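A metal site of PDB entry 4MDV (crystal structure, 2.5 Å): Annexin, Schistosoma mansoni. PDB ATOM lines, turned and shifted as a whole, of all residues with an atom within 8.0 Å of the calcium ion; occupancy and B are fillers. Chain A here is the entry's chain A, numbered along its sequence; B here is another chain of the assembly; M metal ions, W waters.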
ATOM      1  N   TYR A 118      28.308 -22.765 -18.127  1.00  0.00           N
ATOM      2  CA  TYR A 118      28.681 -22.858 -19.527  1.00  0.00           C
ATOM      3  C   TYR A 118      29.016 -24.297 -19.922  1.00  0.00           C
ATOM      4  O   TYR A 118      28.511 -24.820 -20.916  1.00  0.00           O
ATOM      5  CB  TYR A 118      29.858 -21.930 -19.784  1.00  0.00           C
ATOM      6  CG  TYR A 118      30.534 -22.099 -21.129  1.00  0.00           C
ATOM      7  CD1 TYR A 118      30.111 -21.377 -22.245  1.00  0.00           C
ATOM      8  CD2 TYR A 118      31.623 -22.959 -21.283  1.00  0.00           C
ATOM      9  CE1 TYR A 118      30.741 -21.515 -23.471  1.00  0.00           C
ATOM     10  CE2 TYR A 118      32.260 -23.101 -22.497  1.00  0.00           C
ATOM     11  CZ  TYR A 118      31.814 -22.388 -23.587  1.00  0.00           C
ATOM     12  OH  TYR A 118      32.458 -22.531 -24.780  1.00  0.00           O
ATOM     13  N   TYR A 119      29.859 -24.963 -19.129  1.00  0.00           N
ATOM     14  CA  TYR A 119      30.196 -26.341 -19.462  1.00  0.00           C
ATOM     15  C   TYR A 119      29.022 -27.305 -19.277  1.00  0.00           C
ATOM     16  O   TYR A 119      28.953 -28.335 -19.943  1.00  0.00           O
ATOM     17  CB  TYR A 119      31.478 -26.788 -18.745  1.00  0.00           C
ATOM     18  CG  TYR A 119      32.730 -26.193 -19.351  1.00  0.00           C
ATOM     19  CD1 TYR A 119      33.054 -26.411 -20.701  1.00  0.00           C
ATOM     20  CD2 TYR A 119      33.586 -25.381 -18.604  1.00  0.00           C
ATOM     21  CE1 TYR A 119      34.184 -25.855 -21.264  1.00  0.00           C
ATOM     22  CE2 TYR A 119      34.732 -24.811 -19.164  1.00  0.00           C
ATOM     23  CZ  TYR A 119      35.030 -25.058 -20.501  1.00  0.00           C
ATOM     24  OH  TYR A 119      36.178 -24.519 -21.080  1.00  0.00           O
ATOM     25  N   ALA A 120      28.087 -26.945 -18.406  1.00  0.00           N
ATOM     26  CA  ALA A 120      26.895 -27.753 -18.183  1.00  0.00           C
ATOM     27  C   ALA A 120      26.016 -27.786 -19.427  1.00  0.00           C
ATOM     28  O   ALA A 120      25.243 -28.727 -19.658  1.00  0.00           O
ATOM     29  CB  ALA A 120      26.120 -27.244 -16.993  1.00  0.00           C
ATOM     30  N   MET A 121      26.131 -26.752 -20.253  1.00  0.00           N
ATOM     31  CA  MET A 121      25.247 -26.640 -21.402  1.00  0.00           C
ATOM     32  C   MET A 121      25.996 -26.888 -22.721  1.00  0.00           C
ATOM     33  O   MET A 121      25.440 -27.501 -23.635  1.00  0.00           O
ATOM     34  CB  MET A 121      24.526 -25.297 -21.387  1.00  0.00           C
ATOM     35  CG  MET A 121      23.707 -25.129 -20.108  1.00  0.00           C
ATOM     36  SD  MET A 121      22.669 -23.675 -20.203  1.00  0.00           S
ATOM     37  CE  MET A 121      23.923 -22.391 -20.043  1.00  0.00           C
ATOM     38  N   LYS A 122      27.247 -26.445 -22.810  1.00  0.00           N
ATOM     39  CA  LYS A 122      28.057 -26.793 -23.944  1.00  0.00           C
ATOM     40  C   LYS A 122      28.167 -28.312 -23.911  1.00  0.00           C
ATOM     41  O   LYS A 122      28.193 -28.924 -22.846  1.00  0.00           O
ATOM     42  CB  LYS A 122      29.425 -26.115 -23.872  1.00  0.00           C
ATOM     43  N   GLY A 123      28.186 -28.924 -25.083  1.00  0.00           N
ATOM     44  CA  GLY A 123      28.237 -30.374 -25.137  1.00  0.00           C
ATOM     45  C   GLY A 123      26.893 -30.998 -25.456  1.00  0.00           C
ATOM     46  O   GLY A 123      25.874 -30.323 -25.472  1.00  0.00           O
ATOM     47  N   LEU A 124      26.899 -32.298 -25.736  1.00  0.00           N
ATOM     48  CA  LEU A 124      25.660 -32.984 -26.048  1.00  0.00           C
ATOM     49  C   LEU A 124      24.899 -33.238 -24.763  1.00  0.00           C
ATOM     50  O   LEU A 124      25.480 -33.664 -23.746  1.00  0.00           O
ATOM     51  CB  LEU A 124      25.933 -34.286 -26.791  1.00  0.00           C
ATOM     52  CG  LEU A 124      26.528 -34.091 -28.184  1.00  0.00           C
ATOM     53  CD1 LEU A 124      27.084 -35.409 -28.723  1.00  0.00           C
ATOM     54  CD2 LEU A 124      25.503 -33.487 -29.136  1.00  0.00           C
ATOM     55  N   GLY A 125      23.598 -32.959 -24.816  1.00  0.00           N
ATOM     56  CA  GLY A 125      22.757 -33.095 -23.657  1.00  0.00           C
ATOM     57  C   GLY A 125      22.938 -31.899 -22.749  1.00  0.00           C
ATOM     58  O   GLY A 125      23.512 -30.890 -23.142  1.00  0.00           O
ATOM     59  N   THR A 126      22.448 -32.035 -21.535  1.00  0.00           N
ATOM     60  CA  THR A 126      22.450 -30.916 -20.609  1.00  0.00           C
ATOM     61  C   THR A 126      22.680 -31.453 -19.241  1.00  0.00           C
ATOM     62  O   THR A 126      21.963 -32.332 -18.793  1.00  0.00           O
ATOM     63  CB  THR A 126      21.100 -30.201 -20.610  1.00  0.00           C
ATOM     64  OG1 THR A 126      20.760 -29.807 -21.961  1.00  0.00           O
ATOM     65  CG2 THR A 126      21.172 -28.973 -19.709  1.00  0.00           C
ATOM     66  N   ASN A 127      23.714 -30.951 -18.580  1.00  0.00           N
ATOM     67  CA  ASN A 127      23.953 -31.310 -17.205  1.00  0.00           C
ATOM     68  C   ASN A 127      22.992 -30.587 -16.278  1.00  0.00           C
ATOM     69  O   ASN A 127      23.349 -29.592 -15.636  1.00  0.00           O
ATOM     70  CB  ASN A 127      25.359 -30.993 -16.816  1.00  0.00           C
ATOM     71  CG  ASN A 127      25.824 -31.888 -15.733  1.00  0.00           C
ATOM     72  OD1 ASN A 127      25.021 -32.327 -14.900  1.00  0.00           O
ATOM     73  ND2 ASN A 127      27.112 -32.206 -15.729  1.00  0.00           N
ATOM     74  N   ASP A 169      21.254 -19.190 -23.833  1.00  0.00           N
ATOM     75  CA  ASP A 169      21.722 -20.582 -23.772  1.00  0.00           C
ATOM     76  C   ASP A 169      20.766 -21.546 -23.074  1.00  0.00           C
ATOM     77  O   ASP A 169      20.548 -22.652 -23.585  1.00  0.00           O
ATOM     78  CB  ASP A 169      23.135 -20.683 -23.171  1.00  0.00           C
ATOM     79  CG  ASP A 169      24.231 -20.305 -24.190  1.00  0.00           C
ATOM     80  OD1 ASP A 169      23.883 -19.771 -25.261  1.00  0.00           O
ATOM     81  OD2 ASP A 169      25.422 -20.543 -23.922  1.00  0.00           O
ATOM     82  N   LYS A 172      17.470 -22.385 -25.182  1.00  0.00           N
ATOM     83  CA  LYS A 172      17.802 -23.353 -26.226  1.00  0.00           C
ATOM     84  C   LYS A 172      18.046 -24.731 -25.611  1.00  0.00           C
ATOM     85  O   LYS A 172      17.768 -25.772 -26.219  1.00  0.00           O
ATOM     86  CB  LYS A 172      19.029 -22.908 -27.032  1.00  0.00           C
ATOM     87  N   GLU A 173      18.544 -24.709 -24.385  1.00  0.00           N
ATOM     88  CA  GLU A 173      18.985 -25.891 -23.674  1.00  0.00           C
ATOM     89  C   GLU A 173      17.834 -26.612 -22.971  1.00  0.00           C
ATOM     90  O   GLU A 173      17.925 -27.806 -22.664  1.00  0.00           O
ATOM     91  CB  GLU A 173      20.013 -25.449 -22.636  1.00  0.00           C
ATOM     92  CG  GLU A 173      20.949 -26.521 -22.176  1.00  0.00           C
ATOM     93  CD  GLU A 173      21.826 -27.019 -23.291  1.00  0.00           C
ATOM     94  OE1 GLU A 173      22.009 -26.270 -24.270  1.00  0.00           O
ATOM     95  OE2 GLU A 173      22.331 -28.149 -23.191  1.00  0.00           O
ATOM     96  N   GLY B 176      15.979 -30.682 -27.011  1.00  0.00           N
ATOM     97  CA  GLY B 176      17.407 -30.891 -27.120  1.00  0.00           C
ATOM     98  C   GLY B 176      17.855 -32.220 -27.714  1.00  0.00           C
ATOM     99  O   GLY B 176      17.118 -32.876 -28.462  1.00  0.00           O
ATOM    100  N   ASP B 177      19.086 -32.605 -27.392  1.00  0.00           N
ATOM    101  CA  ASP B 177      19.654 -33.849 -27.895  1.00  0.00           C
ATOM    102  C   ASP B 177      18.836 -35.070 -27.462  1.00  0.00           C
ATOM    103  O   ASP B 177      18.594 -35.990 -28.256  1.00  0.00           O
ATOM    104  CB  ASP B 177      21.130 -33.926 -27.522  1.00  0.00           C
ATOM    105  CG  ASP B 177      21.938 -32.815 -28.181  1.00  0.00           C
ATOM    106  OD1 ASP B 177      21.614 -32.530 -29.352  1.00  0.00           O
ATOM    107  OD2 ASP B 177      22.839 -32.209 -27.530  1.00  0.00           O
ATOM    108  N   SER B 273      25.881 -35.485 -21.313  1.00  0.00           N
ATOM    109  CA  SER B 273      25.340 -35.153 -19.984  1.00  0.00           C
ATOM    110  C   SER B 273      23.834 -35.364 -19.904  1.00  0.00           C
ATOM    111  O   SER B 273      23.164 -35.551 -20.920  1.00  0.00           O
ATOM    112  CB  SER B 273      25.695 -33.708 -19.588  1.00  0.00           C
ATOM    113  OG  SER B 273      26.881 -33.657 -18.796  1.00  0.00           O
ATOM    114  N   TYR B 276      20.065 -37.136 -21.974  1.00  0.00           N
ATOM    115  CA  TYR B 276      20.672 -37.629 -23.193  1.00  0.00           C
ATOM    116  C   TYR B 276      21.674 -38.736 -22.874  1.00  0.00           C
ATOM    117  O   TYR B 276      21.561 -39.853 -23.387  1.00  0.00           O
ATOM    118  CB  TYR B 276      21.355 -36.496 -23.971  1.00  0.00           C
ATOM    119  CG  TYR B 276      21.882 -36.910 -25.322  1.00  0.00           C
ATOM    120  CD1 TYR B 276      21.042 -37.513 -26.256  1.00  0.00           C
ATOM    121  CD2 TYR B 276      23.214 -36.724 -25.661  1.00  0.00           C
ATOM    122  CE1 TYR B 276      21.514 -37.909 -27.503  1.00  0.00           C
ATOM    123  CE2 TYR B 276      23.701 -37.115 -26.890  1.00  0.00           C
ATOM    124  CZ  TYR B 276      22.848 -37.709 -27.805  1.00  0.00           C
ATOM    125  OH  TYR B 276      23.327 -38.105 -29.031  1.00  0.00           O
HETATM  126 CA    CA M   1      23.932 -29.094 -24.724  1.00  0.00          CA
HETATM  127  O   HOH W   1      23.833 -27.196 -26.486  1.00  0.00           O
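Of the 17 residues printed, 4 come within 4 Å of the calcium ion. The nearest printed residue that does not touch the calcium ion is Leu 124 (4.3 Å).
The calcium ion is bound by the side-chain carboxylate of Glu 173 (2.4 Å), the backbone carbonyl oxygen of Gly 123 (2.4 Å), the backbone carbonyl oxygen of Gly 125 (2.4 Å), the backbone carbonyl oxygen of Met 121 (2.4 Å) and water W1 (2.6 Å).
The side-chain carboxylate (OE2) of Glu 173 lies close to the side-chain hydroxyl (OG1) of Thr 126 (2.6 Å). The backbone NH (N) of Gly 125 is in hydrogen-bond range of the side-chain carboxylate (OD2) of Asp 177 of chain B (2.9 Å).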
